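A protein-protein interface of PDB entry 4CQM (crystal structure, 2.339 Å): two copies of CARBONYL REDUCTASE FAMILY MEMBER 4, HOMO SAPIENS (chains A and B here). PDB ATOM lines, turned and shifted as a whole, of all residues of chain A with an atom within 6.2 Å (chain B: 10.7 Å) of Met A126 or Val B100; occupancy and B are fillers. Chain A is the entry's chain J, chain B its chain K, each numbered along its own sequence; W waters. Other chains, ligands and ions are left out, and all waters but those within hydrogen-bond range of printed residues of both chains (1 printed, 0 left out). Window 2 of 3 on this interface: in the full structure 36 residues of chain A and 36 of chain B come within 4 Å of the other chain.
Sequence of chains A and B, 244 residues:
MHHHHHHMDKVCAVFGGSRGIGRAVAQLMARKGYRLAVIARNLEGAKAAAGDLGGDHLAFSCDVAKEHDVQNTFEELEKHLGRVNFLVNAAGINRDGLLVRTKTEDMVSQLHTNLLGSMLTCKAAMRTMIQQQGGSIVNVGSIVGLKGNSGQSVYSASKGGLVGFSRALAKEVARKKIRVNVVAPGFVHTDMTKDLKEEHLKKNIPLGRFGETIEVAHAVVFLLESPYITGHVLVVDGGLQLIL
The side-chain carboxylate of Glu A172 is in hydrogen-bond range of the backbone NH of Leu B99 (3.0 Å). The side-chain carboxylate (OE1) of Glu A172 lies within hydrogen-bond range of the backbone NH (N) of Gly B151, at 3.2 Å. The backbone carbonyl oxygen (O) of Thr B102 sits at hydrogen-bond distance from the side-chain amino group (NZ) of Lys A123 (2.9 Å).
The backbone carbonyl oxygen (O) of Leu B98 is in hydrogen-bond range of the side-chain hydroxyl (OG1) of Thr B102 (2.5 Å). The backbone NH (N) of Gly B97 sits at hydrogen-bond distance from the backbone carbonyl oxygen (O) of Gly B151 (2.9 Å).
Leu B99 touches Lys A123 (O to CG, 3.6 Å). NZ of Lys A123 touches CA of Lys B103 (3.8 Å). Val B100 touches Met A126. CD2 of Leu B99 touches CD2 of Leu A169 (3.9 Å). CA of Leu B98 touches OE2 of Glu A172 (3.3 Å). OG of Ser B150 touches CA of Glu A172 (3.3 Å).
No residue of chain B comes within 4 Å of Cys A122. Of the printed residues of chain B, Lys A123 touches Leu B99 (3.6 Å), Thr B102 (2.9 Å) and Lys B103 (3.8 Å). No residue of chain B comes within 4 Å of Ala A124. Ala A125 touches none of the printed residues of chain B. Of chain B, only Val B100 comes within 4 Å of Met A126. No residue of chain B comes within 4 Å of Thr A128. No residue of chain B comes within 4 Å of Ile A130. Of the printed residues of chain B, Glu A172 touches Leu B98 (3.3 Å), Leu B99 (3.0 Å), Ser B150 (3.3 Å) and Gly B151 (3.2 Å). Of the printed residues of chain A, Leu B99 touches Lys A123, Leu A169 and Glu A172. Val B100 touches just one residue of chain A: Met A126 (3.6 Å). Of the printed residues of chain A, Thr B102 touches Lys A123 (2.9 Å). Of the printed residues of chain A, Lys B103 touches Lys A123. Thr B104 touches none of the printed residues of chain A. Printed residues of chain A within 4 Å of Ser B150: Glu A172. The nearest printed residue of chain A that does not touch Gly B151 is Leu A169 (6.7 Å).
Hydrophobic or aromatic side chains of chain B within 4 Å of the printed part of chain A: Leu B98, Leu B99 and Val B100. Hydrophobic or aromatic side chains of chain A within 4 Å of the printed part of chain B: Met A126 and Leu A169. Among the printed residues, no Asp or Glu carboxylate lies within 4 Å of a Lys or Arg side-chain nitrogen of the other chain.
No position is printed for both chains. Of the 9 pairs that touch across the chains among the printed residues, none has its exchanged pair printed and touching as well.
Water W1 lies within hydrogen-bond range of the side-chain carboxylate of Glu A172 (2.4 Å), the backbone carbonyl oxygen of Gly B97 (2.6 Å), the side-chain hydroxyl of Ser B153 (2.8 Å) and the backbone NH of Leu B99 (3.5 Å).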
ATOM      1  N   THR A 121     -20.069 -28.981   1.214  1.00  0.00           N
ATOM      2  CA  THR A 121     -18.880 -29.466   0.530  1.00  0.00           C
ATOM      3  C   THR A 121     -18.459 -28.512  -0.583  1.00  0.00           C
ATOM      4  O   THR A 121     -17.281 -28.172  -0.709  1.00  0.00           O
ATOM      5  CB  THR A 121     -19.106 -30.866  -0.061  1.00  0.00           C
ATOM      6  OG1 THR A 121     -19.479 -31.773   0.984  1.00  0.00           O
ATOM      7  CG2 THR A 121     -17.843 -31.365  -0.723  1.00  0.00           C
ATOM      8  N   CYS A 122     -19.426 -28.083  -1.388  1.00  0.00           N
ATOM      9  CA  CYS A 122     -19.164 -27.125  -2.456  1.00  0.00           C
ATOM     10  C   CYS A 122     -18.741 -25.780  -1.883  1.00  0.00           C
ATOM     11  O   CYS A 122     -17.924 -25.074  -2.474  1.00  0.00           O
ATOM     12  CB  CYS A 122     -20.397 -26.953  -3.344  1.00  0.00           C
ATOM     13  SG  CYS A 122     -20.803 -28.398  -4.347  1.00  0.00           S
ATOM     14  N   LYS A 123     -19.302 -25.434  -0.729  1.00  0.00           N
ATOM     15  CA  LYS A 123     -18.994 -24.176  -0.060  1.00  0.00           C
ATOM     16  C   LYS A 123     -17.524 -24.094   0.339  1.00  0.00           C
ATOM     17  O   LYS A 123     -16.866 -23.078   0.113  1.00  0.00           O
ATOM     18  CB  LYS A 123     -19.880 -24.003   1.174  1.00  0.00           C
ATOM     19  CG  LYS A 123     -19.567 -22.770   2.002  1.00  0.00           C
ATOM     20  CD  LYS A 123     -20.423 -22.728   3.256  1.00  0.00           C
ATOM     21  CE  LYS A 123     -20.067 -21.542   4.136  1.00  0.00           C
ATOM     22  NZ  LYS A 123     -20.916 -21.493   5.358  1.00  0.00           N
ATOM     23  N   ALA A 124     -17.015 -25.170   0.931  1.00  0.00           N
ATOM     24  CA  ALA A 124     -15.630 -25.213   1.384  1.00  0.00           C
ATOM     25  C   ALA A 124     -14.668 -25.367   0.210  1.00  0.00           C
ATOM     26  O   ALA A 124     -13.507 -24.965   0.289  1.00  0.00           O
ATOM     27  CB  ALA A 124     -15.434 -26.344   2.379  1.00  0.00           C
ATOM     28  N   ALA A 125     -15.159 -25.949  -0.879  1.00  0.00           N
ATOM     29  CA  ALA A 125     -14.349 -26.139  -2.075  1.00  0.00           C
ATOM     30  C   ALA A 125     -14.135 -24.817  -2.804  1.00  0.00           C
ATOM     31  O   ALA A 125     -13.171 -24.663  -3.552  1.00  0.00           O
ATOM     32  CB  ALA A 125     -14.996 -27.156  -3.001  1.00  0.00           C
ATOM     33  N   MET A 126     -15.041 -23.869  -2.582  1.00  0.00           N
ATOM     34  CA  MET A 126     -14.952 -22.554  -3.210  1.00  0.00           C
ATOM     35  C   MET A 126     -13.657 -21.845  -2.838  1.00  0.00           C
ATOM     36  O   MET A 126     -13.030 -21.204  -3.678  1.00  0.00           O
ATOM     37  CB  MET A 126     -16.148 -21.685  -2.816  1.00  0.00           C
ATOM     38  CG  MET A 126     -17.482 -22.112  -3.413  1.00  0.00           C
ATOM     39  SD  MET A 126     -17.578 -21.904  -5.201  1.00  0.00           S
ATOM     40  CE  MET A 126     -17.224 -23.565  -5.774  1.00  0.00           C
ATOM     41  N   ARG A 127     -13.261 -21.970  -1.575  1.00  0.00           N
ATOM     42  CA  ARG A 127     -12.055 -21.319  -1.079  1.00  0.00           C
ATOM     43  C   ARG A 127     -10.808 -21.799  -1.816  1.00  0.00           C
ATOM     44  O   ARG A 127      -9.985 -20.993  -2.245  1.00  0.00           O
ATOM     45  CB  ARG A 127     -11.899 -21.560   0.424  1.00  0.00           C
ATOM     46  N   THR A 128     -10.679 -23.113  -1.971  1.00  0.00           N
ATOM     47  CA  THR A 128      -9.501 -23.696  -2.605  1.00  0.00           C
ATOM     48  C   THR A 128      -9.525 -23.560  -4.127  1.00  0.00           C
ATOM     49  O   THR A 128      -8.476 -23.499  -4.768  1.00  0.00           O
ATOM     50  CB  THR A 128      -9.349 -25.187  -2.241  1.00  0.00           C
ATOM     51  OG1 THR A 128     -10.567 -25.881  -2.542  1.00  0.00           O
ATOM     52  CG2 THR A 128      -9.035 -25.344  -0.761  1.00  0.00           C
ATOM     53  N   MET A 129     -10.723 -23.513  -4.702  1.00  0.00           N
ATOM     54  CA  MET A 129     -10.863 -23.426  -6.153  1.00  0.00           C
ATOM     55  C   MET A 129     -10.722 -21.992  -6.656  1.00  0.00           C
ATOM     56  O   MET A 129     -10.336 -21.766  -7.804  1.00  0.00           O
ATOM     57  CB  MET A 129     -12.203 -24.014  -6.593  1.00  0.00           C
ATOM     58  CG  MET A 129     -12.255 -25.528  -6.510  1.00  0.00           C
ATOM     59  SD  MET A 129     -13.848 -26.212  -6.984  1.00  0.00           S
ATOM     60  CE  MET A 129     -13.513 -27.962  -6.816  1.00  0.00           C
ATOM     61  N   ILE A 130     -11.035 -21.025  -5.799  1.00  0.00           N
ATOM     62  CA  ILE A 130     -10.813 -19.622  -6.127  1.00  0.00           C
ATOM     63  C   ILE A 130      -9.327 -19.299  -5.985  1.00  0.00           C
ATOM     64  O   ILE A 130      -8.762 -18.548  -6.782  1.00  0.00           O
ATOM     65  CB  ILE A 130     -11.657 -18.689  -5.230  1.00  0.00           C
ATOM     66  CG1 ILE A 130     -13.129 -18.744  -5.646  1.00  0.00           C
ATOM     67  CG2 ILE A 130     -11.160 -17.256  -5.310  1.00  0.00           C
ATOM     68  CD1 ILE A 130     -14.032 -17.852  -4.821  1.00  0.00           C
ATOM     69  N   GLN A 131      -8.691 -19.904  -4.986  1.00  0.00           N
ATOM     70  CA  GLN A 131      -7.265 -19.703  -4.740  1.00  0.00           C
ATOM     71  C   GLN A 131      -6.393 -20.369  -5.803  1.00  0.00           C
ATOM     72  O   GLN A 131      -5.166 -20.283  -5.752  1.00  0.00           O
ATOM     73  CB  GLN A 131      -6.885 -20.227  -3.354  1.00  0.00           C
ATOM     74  CG  GLN A 131      -7.322 -19.327  -2.212  1.00  0.00           C
ATOM     75  CD  GLN A 131      -7.203 -20.001  -0.860  1.00  0.00           C
ATOM     76  OE1 GLN A 131      -6.667 -21.103  -0.749  1.00  0.00           O
ATOM     77  NE2 GLN A 131      -7.709 -19.342   0.176  1.00  0.00           N
ATOM     78  N   ILE A 137     -16.640 -29.286 -10.293  1.00  0.00           N
ATOM     79  CA  ILE A 137     -17.437 -29.997  -9.303  1.00  0.00           C
ATOM     80  C   ILE A 137     -18.496 -30.878  -9.953  1.00  0.00           C
ATOM     81  O   ILE A 137     -19.239 -30.433 -10.829  1.00  0.00           O
ATOM     82  CB  ILE A 137     -18.132 -29.020  -8.332  1.00  0.00           C
ATOM     83  CG1 ILE A 137     -17.109 -28.078  -7.696  1.00  0.00           C
ATOM     84  CG2 ILE A 137     -18.899 -29.782  -7.260  1.00  0.00           C
ATOM     85  CD1 ILE A 137     -17.712 -27.088  -6.728  1.00  0.00           C
ATOM     86  N   LEU A 169     -25.196 -22.388  -8.631  1.00  0.00           N
ATOM     87  CA  LEU A 169     -23.793 -22.212  -8.276  1.00  0.00           C
ATOM     88  C   LEU A 169     -22.931 -22.112  -9.528  1.00  0.00           C
ATOM     89  O   LEU A 169     -21.938 -21.383  -9.550  1.00  0.00           O
ATOM     90  CB  LEU A 169     -23.310 -23.364  -7.392  1.00  0.00           C
ATOM     91  CG  LEU A 169     -21.850 -23.299  -6.936  1.00  0.00           C
ATOM     92  CD1 LEU A 169     -21.582 -22.012  -6.169  1.00  0.00           C
ATOM     93  CD2 LEU A 169     -21.491 -24.513  -6.093  1.00  0.00           C
ATOM     94  N   GLU A 172     -23.120 -18.731 -10.751  1.00  0.00           N
ATOM     95  CA  GLU A 172     -22.564 -17.825  -9.755  1.00  0.00           C
ATOM     96  C   GLU A 172     -21.040 -17.729  -9.821  1.00  0.00           C
ATOM     97  O   GLU A 172     -20.463 -16.693  -9.490  1.00  0.00           O
ATOM     98  CB  GLU A 172     -23.002 -18.270  -8.355  1.00  0.00           C
ATOM     99  CG  GLU A 172     -22.509 -17.391  -7.216  1.00  0.00           C
ATOM    100  CD  GLU A 172     -23.063 -17.818  -5.869  1.00  0.00           C
ATOM    101  OE1 GLU A 172     -24.280 -18.088  -5.783  1.00  0.00           O
ATOM    102  OE2 GLU A 172     -22.283 -17.882  -4.895  1.00  0.00           O
ATOM    103  N   VAL A 173     -20.390 -18.800 -10.264  1.00  0.00           N
ATOM    104  CA  VAL A 173     -18.936 -18.879 -10.180  1.00  0.00           C
ATOM    105  C   VAL A 173     -18.292 -19.283 -11.518  1.00  0.00           C
ATOM    106  O   VAL A 173     -17.104 -19.611 -11.582  1.00  0.00           O
ATOM    107  CB  VAL A 173     -18.521 -19.867  -9.055  1.00  0.00           C
ATOM    108  CG1 VAL A 173     -18.663 -21.315  -9.515  1.00  0.00           C
ATOM    109  CG2 VAL A 173     -17.114 -19.567  -8.543  1.00  0.00           C
ATOM    110  N   ILE A 178     -14.743 -21.960 -12.685  1.00  0.00           N
ATOM    111  CA  ILE A 178     -15.192 -23.092 -11.885  1.00  0.00           C
ATOM    112  C   ILE A 178     -16.477 -23.676 -12.453  1.00  0.00           C
ATOM    113  O   ILE A 178     -17.503 -22.998 -12.524  1.00  0.00           O
ATOM    114  CB  ILE A 178     -15.413 -22.693 -10.418  1.00  0.00           C
ATOM    115  CG1 ILE A 178     -14.107 -22.189  -9.801  1.00  0.00           C
ATOM    116  CG2 ILE A 178     -15.958 -23.869  -9.623  1.00  0.00           C
ATOM    117  CD1 ILE A 178     -14.248 -21.722  -8.374  1.00  0.00           C
ATOM    118  N   VAL A 180     -19.587 -26.469 -12.445  1.00  0.00           N
ATOM    119  CA  VAL A 180     -20.386 -27.324 -11.574  1.00  0.00           C
ATOM    120  C   VAL A 180     -21.381 -28.132 -12.402  1.00  0.00           C
ATOM    121  O   VAL A 180     -22.154 -27.570 -13.177  1.00  0.00           O
ATOM    122  CB  VAL A 180     -21.147 -26.508 -10.512  1.00  0.00           C
ATOM    123  CG1 VAL A 180     -21.775 -27.435  -9.483  1.00  0.00           C
ATOM    124  CG2 VAL A 180     -20.216 -25.514  -9.833  1.00  0.00           C
ATOM    125  N   ARG B  95     -33.362 -15.261   1.084  1.00  0.00           N
ATOM    126  CA  ARG B  95     -32.303 -14.308   1.378  1.00  0.00           C
ATOM    127  C   ARG B  95     -31.145 -14.521   0.410  1.00  0.00           C
ATOM    128  O   ARG B  95     -30.373 -15.469   0.553  1.00  0.00           O
ATOM    129  CB  ARG B  95     -31.823 -14.444   2.824  1.00  0.00           C
ATOM    130  CG  ARG B  95     -30.700 -13.486   3.192  1.00  0.00           C
ATOM    131  CD  ARG B  95     -30.331 -13.595   4.663  1.00  0.00           C
ATOM    132  NE  ARG B  95     -29.273 -12.657   5.027  1.00  0.00           N
ATOM    133  CZ  ARG B  95     -28.820 -12.485   6.265  1.00  0.00           C
ATOM    134  NH1 ARG B  95     -29.336 -13.188   7.265  1.00  0.00           N
ATOM    135  NH2 ARG B  95     -27.854 -11.610   6.504  1.00  0.00           N
ATOM    136  N   ASP B  96     -31.038 -13.642  -0.580  1.00  0.00           N
ATOM    137  CA  ASP B  96     -29.996 -13.750  -1.594  1.00  0.00           C
ATOM    138  C   ASP B  96     -28.609 -13.582  -0.986  1.00  0.00           C
ATOM    139  O   ASP B  96     -28.429 -12.844  -0.017  1.00  0.00           O
ATOM    140  CB  ASP B  96     -30.212 -12.717  -2.700  1.00  0.00           C
ATOM    141  CG  ASP B  96     -31.518 -12.922  -3.441  1.00  0.00           C
ATOM    142  OD1 ASP B  96     -32.042 -14.055  -3.422  1.00  0.00           O
ATOM    143  OD2 ASP B  96     -32.020 -11.950  -4.045  1.00  0.00           O
ATOM    144  N   GLY B  97     -27.632 -14.274  -1.561  1.00  0.00           N
ATOM    145  CA  GLY B  97     -26.266 -14.204  -1.083  1.00  0.00           C
ATOM    146  C   GLY B  97     -25.393 -15.287  -1.682  1.00  0.00           C
ATOM    147  O   GLY B  97     -25.877 -16.361  -2.040  1.00  0.00           O
ATOM    148  N   LEU B  98     -24.100 -15.001  -1.796  1.00  0.00           N
ATOM    149  CA  LEU B  98     -23.147 -15.963  -2.329  1.00  0.00           C
ATOM    150  C   LEU B  98     -23.005 -17.153  -1.386  1.00  0.00           C
ATOM    151  O   LEU B  98     -23.148 -17.010  -0.171  1.00  0.00           O
ATOM    152  CB  LEU B  98     -21.787 -15.301  -2.558  1.00  0.00           C
ATOM    153  CG  LEU B  98     -21.783 -14.076  -3.477  1.00  0.00           C
ATOM    154  CD1 LEU B  98     -20.392 -13.467  -3.558  1.00  0.00           C
ATOM    155  CD2 LEU B  98     -22.294 -14.444  -4.862  1.00  0.00           C
ATOM    156  N   LEU B  99     -22.725 -18.324  -1.952  1.00  0.00           N
ATOM    157  CA  LEU B  99     -22.571 -19.542  -1.164  1.00  0.00           C
ATOM    158  C   LEU B  99     -21.424 -19.409  -0.168  1.00  0.00           C
ATOM    159  O   LEU B  99     -21.474 -19.966   0.930  1.00  0.00           O
ATOM    160  CB  LEU B  99     -22.338 -20.747  -2.079  1.00  0.00           C
ATOM    161  CG  LEU B  99     -22.223 -22.108  -1.391  1.00  0.00           C
ATOM    162  CD1 LEU B  99     -23.511 -22.449  -0.655  1.00  0.00           C
ATOM    163  CD2 LEU B  99     -21.869 -23.193  -2.396  1.00  0.00           C
ATOM    164  N   VAL B 100     -20.396 -18.665  -0.557  1.00  0.00           N
ATOM    165  CA  VAL B 100     -19.253 -18.420   0.312  1.00  0.00           C
ATOM    166  C   VAL B 100     -19.654 -17.521   1.482  1.00  0.00           C
ATOM    167  O   VAL B 100     -19.147 -17.671   2.596  1.00  0.00           O
ATOM    168  CB  VAL B 100     -18.072 -17.797  -0.480  1.00  0.00           C
ATOM    169  CG1 VAL B 100     -17.510 -16.562   0.218  1.00  0.00           C
ATOM    170  CG2 VAL B 100     -16.981 -18.834  -0.706  1.00  0.00           C
ATOM    171  N   ARG B 101     -20.586 -16.605   1.232  1.00  0.00           N
ATOM    172  CA  ARG B 101     -21.044 -15.687   2.269  1.00  0.00           C
ATOM    173  C   ARG B 101     -22.402 -16.101   2.827  1.00  0.00           C
ATOM    174  O   ARG B 101     -23.226 -15.252   3.166  1.00  0.00           O
ATOM    175  CB  ARG B 101     -21.125 -14.258   1.730  1.00  0.00           C
ATOM    176  CG  ARG B 101     -19.915 -13.816   0.926  1.00  0.00           C
ATOM    177  CD  ARG B 101     -19.888 -12.303   0.784  1.00  0.00           C
ATOM    178  NE  ARG B 101     -19.187 -11.872  -0.422  1.00  0.00           N
ATOM    179  CZ  ARG B 101     -18.868 -10.610  -0.687  1.00  0.00           C
ATOM    180  NH1 ARG B 101     -19.176  -9.651   0.176  1.00  0.00           N
ATOM    181  NH2 ARG B 101     -18.233 -10.306  -1.810  1.00  0.00           N
ATOM    182  N   THR B 102     -22.633 -17.406   2.920  1.00  0.00           N
ATOM    183  CA  THR B 102     -23.887 -17.918   3.459  1.00  0.00           C
ATOM    184  C   THR B 102     -23.636 -18.941   4.560  1.00  0.00           C
ATOM    185  O   THR B 102     -23.185 -20.055   4.293  1.00  0.00           O
ATOM    186  CB  THR B 102     -24.753 -18.560   2.362  1.00  0.00           C
ATOM    187  OG1 THR B 102     -25.056 -17.584   1.357  1.00  0.00           O
ATOM    188  CG2 THR B 102     -26.049 -19.087   2.954  1.00  0.00           C
ATOM    189  N   LYS B 103     -23.932 -18.556   5.798  1.00  0.00           N
ATOM    190  CA  LYS B 103     -23.726 -19.435   6.943  1.00  0.00           C
ATOM    191  C   LYS B 103     -24.749 -20.567   6.963  1.00  0.00           C
ATOM    192  O   LYS B 103     -25.852 -20.431   6.431  1.00  0.00           O
ATOM    193  CB  LYS B 103     -23.779 -18.636   8.249  1.00  0.00           C
ATOM    194  CG  LYS B 103     -24.993 -17.730   8.384  1.00  0.00           C
ATOM    195  CD  LYS B 103     -24.807 -16.723   9.511  1.00  0.00           C
ATOM    196  CE  LYS B 103     -25.963 -15.736   9.575  1.00  0.00           C
ATOM    197  NZ  LYS B 103     -25.722 -14.664  10.580  1.00  0.00           N
ATOM    198  N   THR B 104     -24.364 -21.680   7.581  1.00  0.00           N
ATOM    199  CA  THR B 104     -25.165 -22.903   7.590  1.00  0.00           C
ATOM    200  C   THR B 104     -26.568 -22.683   8.150  1.00  0.00           C
ATOM    201  O   THR B 104     -27.530 -23.298   7.687  1.00  0.00           O
ATOM    202  CB  THR B 104     -24.468 -24.011   8.409  1.00  0.00           C
ATOM    203  OG1 THR B 104     -23.113 -24.157   7.966  1.00  0.00           O
ATOM    204  CG2 THR B 104     -25.194 -25.339   8.253  1.00  0.00           C
ATOM    205  N   ASP B 106     -28.611 -20.207   7.832  1.00  0.00           N
ATOM    206  CA  ASP B 106     -29.515 -19.746   6.785  1.00  0.00           C
ATOM    207  C   ASP B 106     -29.781 -20.848   5.766  1.00  0.00           C
ATOM    208  O   ASP B 106     -30.872 -20.934   5.203  1.00  0.00           O
ATOM    209  CB  ASP B 106     -28.946 -18.510   6.086  1.00  0.00           C
ATOM    210  CG  ASP B 106     -28.930 -17.288   6.984  1.00  0.00           C
ATOM    211  OD1 ASP B 106     -29.821 -17.176   7.851  1.00  0.00           O
ATOM    212  OD2 ASP B 106     -28.028 -16.439   6.821  1.00  0.00           O
ATOM    213  N   MET B 107     -28.776 -21.687   5.534  1.00  0.00           N
ATOM    214  CA  MET B 107     -28.905 -22.803   4.603  1.00  0.00           C
ATOM    215  C   MET B 107     -29.916 -23.825   5.111  1.00  0.00           C
ATOM    216  O   MET B 107     -30.757 -24.307   4.355  1.00  0.00           O
ATOM    217  CB  MET B 107     -27.546 -23.468   4.373  1.00  0.00           C
ATOM    218  CG  MET B 107     -26.549 -22.581   3.645  1.00  0.00           C
ATOM    219  SD  MET B 107     -24.865 -23.222   3.661  1.00  0.00           S
ATOM    220  CE  MET B 107     -25.113 -24.840   2.944  1.00  0.00           C
ATOM    221  N   SER B 150     -27.766 -16.965 -10.128  1.00  0.00           N
ATOM    222  CA  SER B 150     -26.630 -16.499  -9.341  1.00  0.00           C
ATOM    223  C   SER B 150     -27.086 -15.754  -8.091  1.00  0.00           C
ATOM    224  O   SER B 150     -27.981 -14.911  -8.150  1.00  0.00           O
ATOM    225  CB  SER B 150     -25.724 -15.603 -10.186  1.00  0.00           C
ATOM    226  OG  SER B 150     -24.586 -15.189  -9.450  1.00  0.00           O
ATOM    227  N   GLY B 151     -26.465 -16.073  -6.959  1.00  0.00           N
ATOM    228  CA  GLY B 151     -26.803 -15.444  -5.696  1.00  0.00           C
ATOM    229  C   GLY B 151     -28.054 -16.026  -5.065  1.00  0.00           C
ATOM    230  O   GLY B 151     -28.564 -15.497  -4.076  1.00  0.00           O
ATOM    231  N   GLN B 152     -28.550 -17.118  -5.637  1.00  0.00           N
ATOM    232  CA  GLN B 152     -29.757 -17.765  -5.136  1.00  0.00           C
ATOM    233  C   GLN B 152     -29.602 -19.282  -5.083  1.00  0.00           C
ATOM    234  O   GLN B 152     -30.544 -20.016  -5.375  1.00  0.00           O
ATOM    235  CB  GLN B 152     -30.962 -17.400  -6.008  1.00  0.00           C
ATOM    236  CG  GLN B 152     -31.356 -15.935  -5.956  1.00  0.00           C
ATOM    237  CD  GLN B 152     -32.569 -15.628  -6.812  1.00  0.00           C
ATOM    238  OE1 GLN B 152     -32.921 -16.395  -7.709  1.00  0.00           O
ATOM    239  NE2 GLN B 152     -33.218 -14.502  -6.537  1.00  0.00           N
ATOM    240  N   SER B 153     -28.414 -19.743  -4.706  1.00  0.00           N
ATOM    241  CA  SER B 153     -28.116 -21.173  -4.683  1.00  0.00           C
ATOM    242  C   SER B 153     -28.980 -21.923  -3.673  1.00  0.00           C
ATOM    243  O   SER B 153     -29.600 -22.933  -4.005  1.00  0.00           O
ATOM    244  CB  SER B 153     -26.635 -21.405  -4.376  1.00  0.00           C
ATOM    245  OG  SER B 153     -26.289 -20.894  -3.101  1.00  0.00           O
ATOM    246  N   VAL B 154     -29.011 -21.422  -2.442  1.00  0.00           N
ATOM    247  CA  VAL B 154     -29.778 -22.050  -1.371  1.00  0.00           C
ATOM    248  C   VAL B 154     -31.267 -22.071  -1.704  1.00  0.00           C
ATOM    249  O   VAL B 154     -31.948 -23.076  -1.497  1.00  0.00           O
ATOM    250  CB  VAL B 154     -29.564 -21.324  -0.027  1.00  0.00           C
ATOM    251  CG1 VAL B 154     -30.313 -22.036   1.090  1.00  0.00           C
ATOM    252  CG2 VAL B 154     -28.081 -21.233   0.295  1.00  0.00           C
HETATM  253  O   HOH W   1     -25.656 -18.226  -3.817  1.00  0.00           O
